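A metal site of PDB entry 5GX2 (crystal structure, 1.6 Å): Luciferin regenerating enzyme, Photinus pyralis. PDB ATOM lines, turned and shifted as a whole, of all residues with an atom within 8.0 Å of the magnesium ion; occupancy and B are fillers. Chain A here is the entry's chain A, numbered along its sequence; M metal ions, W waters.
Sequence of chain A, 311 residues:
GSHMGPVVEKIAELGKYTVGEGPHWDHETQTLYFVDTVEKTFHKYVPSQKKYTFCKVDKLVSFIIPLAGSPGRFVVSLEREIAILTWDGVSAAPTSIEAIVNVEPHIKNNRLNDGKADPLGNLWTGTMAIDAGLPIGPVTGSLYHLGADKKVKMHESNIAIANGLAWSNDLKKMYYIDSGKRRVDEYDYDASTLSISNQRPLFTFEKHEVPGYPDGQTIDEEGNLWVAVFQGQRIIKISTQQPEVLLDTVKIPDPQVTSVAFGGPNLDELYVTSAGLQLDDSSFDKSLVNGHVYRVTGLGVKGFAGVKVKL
The side-chain amide nitrogen (ND2) of Asn 113 lies close to the side-chain amide oxygen (OD1) of Asn 163, 3.4 Å away.
The side-chain amide nitrogen (ND2) of Asn 163 lies within hydrogen-bond range of the side-chain hydroxyl (OG) of Ser 179, at 2.7 Å.
N of Asn 163 sits at hydrogen-bond distance from O of Ile 177 (2.8 Å).
The backbone NH of Gly 164 sits at hydrogen-bond distance from the backbone carbonyl oxygen of Asp 215, at 2.9 Å.
O of Ala 228 is in hydrogen-bond range of N of Asp 215 (3.0 Å).
The nearest printed residue that does not touch the magnesium ion is Asn 113 (4.1 Å).
The magnesium ion is bound by OE1 of Glu 21 (2.0 Å), water W3 (2.1 Å), OD1 of Asn 163 (2.1 Å), OD1 of Asp 215 (2.1 Å), water W2 (2.2 Å) and water W1 (2.2 Å).
The magnesium ion has six donor atoms within binding distance.
Water W1 lies within hydrogen-bond range of OD1 of Asn 113 and OE2 of Glu 21.
Water W2 lies within hydrogen-bond range of ND2 of Asn 113 (3.0 Å) and ND2 of Asn 163 (3.3 Å).
Water W3 lies within hydrogen-bond range of OE2 of Glu 21 (2.7 Å), OD2 of Asp 114 (2.9 Å) and N of Gly 216 (3.4 Å).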
ATOM      1  N   VAL A  19       2.988 -10.419   3.849  1.00  0.00           N
ATOM      2  CA  VAL A  19       2.812 -10.621   2.411  1.00  0.00           C
ATOM      3  C   VAL A  19       3.790 -11.705   1.976  1.00  0.00           C
ATOM      4  O   VAL A  19       4.901 -11.401   1.526  1.00  0.00           O
ATOM      5  CB  VAL A  19       3.003  -9.345   1.575  1.00  0.00           C
ATOM      6  CG1 VAL A  19       2.642  -9.620   0.110  1.00  0.00           C
ATOM      7  CG2 VAL A  19       2.154  -8.173   2.112  1.00  0.00           C
ATOM      8  N   GLY A  20       3.431 -12.972   2.169  1.00  0.00           N
ATOM      9  CA  GLY A  20       4.243 -14.048   1.629  1.00  0.00           C
ATOM     10  C   GLY A  20       4.249 -13.965   0.113  1.00  0.00           C
ATOM     11  O   GLY A  20       3.243 -13.599  -0.506  1.00  0.00           O
ATOM     12  N   GLU A  21       5.399 -14.267  -0.501  1.00  0.00           N
ATOM     13  CA  GLU A  21       5.607 -13.941  -1.916  1.00  0.00           C
ATOM     14  C   GLU A  21       6.805 -14.699  -2.477  1.00  0.00           C
ATOM     15  O   GLU A  21       7.575 -15.327  -1.755  1.00  0.00           O
ATOM     16  CB  GLU A  21       5.848 -12.425  -2.121  1.00  0.00           C
ATOM     17  CG  GLU A  21       4.621 -11.642  -2.591  1.00  0.00           C
ATOM     18  CD  GLU A  21       4.277 -11.874  -4.048  1.00  0.00           C
ATOM     19  OE1 GLU A  21       3.438 -11.132  -4.587  1.00  0.00           O
ATOM     20  OE2 GLU A  21       4.825 -12.818  -4.655  1.00  0.00           O
ATOM     21  N   GLY A  22       6.954 -14.616  -3.808  1.00  0.00           N
ATOM     22  CA  GLY A  22       8.132 -15.084  -4.508  1.00  0.00           C
ATOM     23  C   GLY A  22       8.558 -16.521  -4.254  1.00  0.00           C
ATOM     24  O   GLY A  22       9.750 -16.802  -4.068  1.00  0.00           O
ATOM     25  N   PRO A  23       7.634 -17.469  -4.284  1.00  0.00           N
ATOM     26  CA  PRO A  23       8.027 -18.875  -4.050  1.00  0.00           C
ATOM     27  C   PRO A  23       8.932 -19.398  -5.156  1.00  0.00           C
ATOM     28  O   PRO A  23       8.696 -19.146  -6.343  1.00  0.00           O
ATOM     29  CB  PRO A  23       6.700 -19.627  -4.023  1.00  0.00           C
ATOM     30  CG  PRO A  23       5.789 -18.798  -4.888  1.00  0.00           C
ATOM     31  CD  PRO A  23       6.191 -17.361  -4.598  1.00  0.00           C
ATOM     32  N   THR A  37       7.332  -9.574   1.369  1.00  0.00           N
ATOM     33  CA  THR A  37       7.710  -8.330   0.710  1.00  0.00           C
ATOM     34  C   THR A  37       7.571  -7.111   1.609  1.00  0.00           C
ATOM     35  O   THR A  37       8.031  -6.030   1.212  1.00  0.00           O
ATOM     36  CB  THR A  37       6.877  -8.091  -0.561  1.00  0.00           C
ATOM     37  OG1 THR A  37       5.480  -8.190  -0.266  1.00  0.00           O
ATOM     38  CG2 THR A  37       7.245  -9.085  -1.637  1.00  0.00           C
ATOM     39  N   SER A  62      11.939  -8.905  -2.448  1.00  0.00           N
ATOM     40  CA  SER A  62      10.820  -9.384  -3.268  1.00  0.00           C
ATOM     41  C   SER A  62      11.068 -10.683  -4.034  1.00  0.00           C
ATOM     42  O   SER A  62      10.095 -11.226  -4.558  1.00  0.00           O
ATOM     43  CB  SER A  62      10.409  -8.284  -4.257  1.00  0.00           C
ATOM     44  OG  SER A  62      11.464  -7.976  -5.159  1.00  0.00           O
ATOM     45  N   ASN A 113       9.981  -5.552  -7.377  1.00  0.00           N
ATOM     46  CA  ASN A 113       8.927  -6.472  -6.984  1.00  0.00           C
ATOM     47  C   ASN A 113       9.185  -7.846  -7.620  1.00  0.00           C
ATOM     48  O   ASN A 113      10.278  -8.385  -7.452  1.00  0.00           O
ATOM     49  CB  ASN A 113       7.532  -5.942  -7.319  1.00  0.00           C
ATOM     50  CG  ASN A 113       6.435  -6.654  -6.539  1.00  0.00           C
ATOM     51  OD1 ASN A 113       6.696  -7.218  -5.466  1.00  0.00           O
ATOM     52  ND2 ASN A 113       5.209  -6.634  -7.052  1.00  0.00           N
ATOM     53  N   ASP A 114       8.223  -8.429  -8.341  1.00  0.00           N
ATOM     54  CA  ASP A 114       8.387  -9.838  -8.668  1.00  0.00           C
ATOM     55  C   ASP A 114       9.555 -10.044  -9.648  1.00  0.00           C
ATOM     56  O   ASP A 114       9.886  -9.158 -10.455  1.00  0.00           O
ATOM     57  CB  ASP A 114       7.085 -10.416  -9.237  1.00  0.00           C
ATOM     58  CG  ASP A 114       6.913 -11.906  -8.959  1.00  0.00           C
ATOM     59  OD1 ASP A 114       7.802 -12.511  -8.326  1.00  0.00           O
ATOM     60  OD2 ASP A 114       5.881 -12.475  -9.390  1.00  0.00           O
ATOM     61  N   GLY A 115      10.208 -11.195  -9.530  1.00  0.00           N
ATOM     62  CA  GLY A 115      11.357 -11.518 -10.359  1.00  0.00           C
ATOM     63  C   GLY A 115      11.445 -13.021 -10.519  1.00  0.00           C
ATOM     64  O   GLY A 115      11.023 -13.785  -9.644  1.00  0.00           O
ATOM     65  N   MET A 128       8.233  -0.833  -8.977  1.00  0.00           N
ATOM     66  CA  MET A 128       6.977  -0.211  -8.608  1.00  0.00           C
ATOM     67  C   MET A 128       7.260   0.868  -7.567  1.00  0.00           C
ATOM     68  O   MET A 128       8.278   0.829  -6.869  1.00  0.00           O
ATOM     69  CB  MET A 128       5.989  -1.233  -8.022  1.00  0.00           C
ATOM     70  CG  MET A 128       6.482  -1.797  -6.685  1.00  0.00           C
ATOM     71  SD  MET A 128       5.485  -3.157  -5.972  1.00  0.00           S
ATOM     72  CE  MET A 128       4.216  -2.226  -5.106  1.00  0.00           C
ATOM     73  N   ILE A 161       2.263  -2.108 -10.760  1.00  0.00           N
ATOM     74  CA  ILE A 161       2.744  -3.107  -9.810  1.00  0.00           C
ATOM     75  C   ILE A 161       3.332  -4.272 -10.606  1.00  0.00           C
ATOM     76  O   ILE A 161       2.604  -5.137 -11.099  1.00  0.00           O
ATOM     77  CB  ILE A 161       1.647  -3.565  -8.832  1.00  0.00           C
ATOM     78  CG1 ILE A 161       1.115  -2.372  -8.024  1.00  0.00           C
ATOM     79  CG2 ILE A 161       2.200  -4.619  -7.869  1.00  0.00           C
ATOM     80  CD1 ILE A 161       0.069  -2.744  -6.982  1.00  0.00           C
ATOM     81  N   ALA A 162       4.663  -4.284 -10.736  1.00  0.00           N
ATOM     82  CA  ALA A 162       5.374  -5.292 -11.516  1.00  0.00           C
ATOM     83  C   ALA A 162       5.210  -6.676 -10.900  1.00  0.00           C
ATOM     84  O   ALA A 162       5.657  -6.917  -9.773  1.00  0.00           O
ATOM     85  CB  ALA A 162       6.858  -4.910 -11.573  1.00  0.00           C
ATOM     86  N   ASN A 163       4.615  -7.610 -11.639  1.00  0.00           N
ATOM     87  CA  ASN A 163       4.304  -8.884 -10.991  1.00  0.00           C
ATOM     88  C   ASN A 163       4.649 -10.103 -11.842  1.00  0.00           C
ATOM     89  O   ASN A 163       5.744 -10.145 -12.401  1.00  0.00           O
ATOM     90  CB  ASN A 163       2.851  -8.862 -10.508  1.00  0.00           C
ATOM     91  CG  ASN A 163       2.775  -8.764  -9.000  1.00  0.00           C
ATOM     92  OD1 ASN A 163       3.582  -9.387  -8.321  1.00  0.00           O
ATOM     93  ND2 ASN A 163       1.854  -7.964  -8.470  1.00  0.00           N
ATOM     94  N   GLY A 164       3.785 -11.132 -11.884  1.00  0.00           N
ATOM     95  CA  GLY A 164       4.235 -12.469 -12.263  1.00  0.00           C
ATOM     96  C   GLY A 164       4.749 -12.597 -13.686  1.00  0.00           C
ATOM     97  O   GLY A 164       4.289 -11.924 -14.618  1.00  0.00           O
ATOM     98  N   ILE A 177       2.527  -9.781 -15.961  1.00  0.00           N
ATOM     99  CA  ILE A 177       1.414  -9.195 -15.207  1.00  0.00           C
ATOM    100  C   ILE A 177       1.850  -7.866 -14.590  1.00  0.00           C
ATOM    101  O   ILE A 177       2.810  -7.824 -13.813  1.00  0.00           O
ATOM    102  CB  ILE A 177       0.917 -10.143 -14.107  1.00  0.00           C
ATOM    103  CG1 ILE A 177       0.240 -11.375 -14.708  1.00  0.00           C
ATOM    104  CG2 ILE A 177      -0.024  -9.385 -13.136  1.00  0.00           C
ATOM    105  CD1 ILE A 177       0.175 -12.559 -13.746  1.00  0.00           C
ATOM    106  N   SER A 179      -0.303  -5.745 -12.082  1.00  0.00           N
ATOM    107  CA  SER A 179      -1.563  -5.968 -11.376  1.00  0.00           C
ATOM    108  C   SER A 179      -2.576  -4.878 -11.680  1.00  0.00           C
ATOM    109  O   SER A 179      -3.783  -5.157 -11.742  1.00  0.00           O
ATOM    110  CB  SER A 179      -1.315  -6.061  -9.873  1.00  0.00           C
ATOM    111  OG  SER A 179      -0.543  -7.194  -9.547  1.00  0.00           O
ATOM    112  N   PRO A 214      -4.563  -9.901 -10.774  1.00  0.00           N
ATOM    113  CA  PRO A 214      -3.518 -10.902 -11.015  1.00  0.00           C
ATOM    114  C   PRO A 214      -2.239 -10.478 -10.299  1.00  0.00           C
ATOM    115  O   PRO A 214      -1.904  -9.294 -10.228  1.00  0.00           O
ATOM    116  CB  PRO A 214      -3.345 -10.889 -12.532  1.00  0.00           C
ATOM    117  CG  PRO A 214      -3.720  -9.489 -12.937  1.00  0.00           C
ATOM    118  CD  PRO A 214      -4.821  -9.061 -11.964  1.00  0.00           C
ATOM    119  N   ASP A 215      -1.533 -11.470  -9.737  1.00  0.00           N
ATOM    120  CA  ASP A 215      -0.344 -11.193  -8.931  1.00  0.00           C
ATOM    121  C   ASP A 215       0.795 -12.039  -9.506  1.00  0.00           C
ATOM    122  O   ASP A 215       1.231 -11.778 -10.625  1.00  0.00           O
ATOM    123  CB  ASP A 215      -0.653 -11.460  -7.445  1.00  0.00           C
ATOM    124  CG  ASP A 215       0.319 -10.763  -6.481  1.00  0.00           C
ATOM    125  OD1 ASP A 215       1.486 -10.546  -6.848  1.00  0.00           O
ATOM    126  OD2 ASP A 215      -0.086 -10.421  -5.350  1.00  0.00           O
ATOM    127  N   GLY A 216       1.256 -13.087  -8.791  1.00  0.00           N
ATOM    128  CA  GLY A 216       2.255 -13.986  -9.364  1.00  0.00           C
ATOM    129  C   GLY A 216       1.635 -14.971 -10.348  1.00  0.00           C
ATOM    130  O   GLY A 216       0.422 -15.180 -10.369  1.00  0.00           O
ATOM    131  N   GLN A 217       2.472 -15.590 -11.187  1.00  0.00           N
ATOM    132  CA  GLN A 217       1.977 -16.666 -12.045  1.00  0.00           C
ATOM    133  C   GLN A 217       3.076 -17.675 -12.337  1.00  0.00           C
ATOM    134  O   GLN A 217       4.270 -17.402 -12.152  1.00  0.00           O
ATOM    135  CB  GLN A 217       1.414 -16.131 -13.373  1.00  0.00           C
ATOM    136  CG  GLN A 217       2.445 -15.512 -14.289  1.00  0.00           C
ATOM    137  CD  GLN A 217       1.832 -14.988 -15.578  1.00  0.00           C
ATOM    138  OE1 GLN A 217       0.803 -15.482 -16.032  1.00  0.00           O
ATOM    139  NE2 GLN A 217       2.475 -13.980 -16.169  1.00  0.00           N
ATOM    140  N   ALA A 228      -2.159 -16.323  -9.584  1.00  0.00           N
ATOM    141  CA  ALA A 228      -2.639 -15.964  -8.254  1.00  0.00           C
ATOM    142  C   ALA A 228      -3.561 -14.759  -8.335  1.00  0.00           C
ATOM    143  O   ALA A 228      -3.257 -13.781  -9.024  1.00  0.00           O
ATOM    144  CB  ALA A 228      -1.454 -15.648  -7.348  1.00  0.00           C
ATOM    145  N   PHE A 230      -5.072 -11.921  -6.209  1.00  0.00           N
ATOM    146  CA  PHE A 230      -5.058 -11.149  -4.972  1.00  0.00           C
ATOM    147  C   PHE A 230      -6.420 -10.484  -4.791  1.00  0.00           C
ATOM    148  O   PHE A 230      -6.884  -9.773  -5.691  1.00  0.00           O
ATOM    149  CB  PHE A 230      -3.932 -10.108  -5.040  1.00  0.00           C
ATOM    150  CG  PHE A 230      -3.664  -9.394  -3.738  1.00  0.00           C
ATOM    151  CD1 PHE A 230      -2.679  -9.847  -2.880  1.00  0.00           C
ATOM    152  CD2 PHE A 230      -4.396  -8.278  -3.373  1.00  0.00           C
ATOM    153  CE1 PHE A 230      -2.421  -9.204  -1.667  1.00  0.00           C
ATOM    154  CE2 PHE A 230      -4.150  -7.630  -2.155  1.00  0.00           C
ATOM    155  CZ  PHE A 230      -3.170  -8.095  -1.315  1.00  0.00           C
ATOM    156  N   VAL A 257      -4.416 -14.123  -2.237  1.00  0.00           N
ATOM    157  CA  VAL A 257      -3.477 -15.045  -2.866  1.00  0.00           C
ATOM    158  C   VAL A 257      -2.437 -14.239  -3.637  1.00  0.00           C
ATOM    159  O   VAL A 257      -2.795 -13.343  -4.412  1.00  0.00           O
ATOM    160  CB  VAL A 257      -4.226 -16.007  -3.793  1.00  0.00           C
ATOM    161  CG1 VAL A 257      -3.259 -17.007  -4.416  1.00  0.00           C
ATOM    162  CG2 VAL A 257      -5.327 -16.730  -3.032  1.00  0.00           C
ATOM    163  N   THR A 258      -1.146 -14.550  -3.433  1.00  0.00           N
ATOM    164  CA  THR A 258      -0.072 -13.720  -3.974  1.00  0.00           C
ATOM    165  C   THR A 258       0.747 -14.385  -5.062  1.00  0.00           C
ATOM    166  O   THR A 258       1.091 -13.716  -6.033  1.00  0.00           O
ATOM    167  CB  THR A 258       0.878 -13.244  -2.868  1.00  0.00           C
ATOM    168  OG1 THR A 258       1.435 -14.385  -2.183  1.00  0.00           O
ATOM    169  CG2 THR A 258       0.138 -12.348  -1.863  1.00  0.00           C
ATOM    170  N   SER A 259       1.115 -15.647  -4.935  1.00  0.00           N
ATOM    171  CA  SER A 259       1.920 -16.257  -5.988  1.00  0.00           C
ATOM    172  C   SER A 259       1.850 -17.775  -5.899  1.00  0.00           C
ATOM    173  O   SER A 259       1.172 -18.342  -5.033  1.00  0.00           O
ATOM    174  CB  SER A 259       3.366 -15.744  -5.925  1.00  0.00           C
ATOM    175  OG  SER A 259       4.038 -16.028  -7.151  1.00  0.00           O
ATOM    176  N   THR A 273       1.388 -18.935  -2.017  1.00  0.00           N
ATOM    177  CA  THR A 273       1.592 -17.960  -0.954  1.00  0.00           C
ATOM    178  C   THR A 273       0.405 -16.997  -0.872  1.00  0.00           C
ATOM    179  O   THR A 273      -0.365 -16.847  -1.833  1.00  0.00           O
ATOM    180  CB  THR A 273       2.886 -17.158  -1.176  1.00  0.00           C
ATOM    181  OG1 THR A 273       2.906 -16.627  -2.503  1.00  0.00           O
ATOM    182  CG2 THR A 273       4.119 -18.051  -0.983  1.00  0.00           C
HETATM  183 MG    MG M   1       3.518 -10.282  -6.432  1.00  0.00          MG
HETATM  184  O   HOH W   1       5.627  -9.845  -6.103  1.00  0.00           O
HETATM  185  O   HOH W   2       3.260  -8.363  -5.486  1.00  0.00           O
HETATM  186  O   HOH W   3       4.059 -12.127  -7.176  1.00  0.00           O
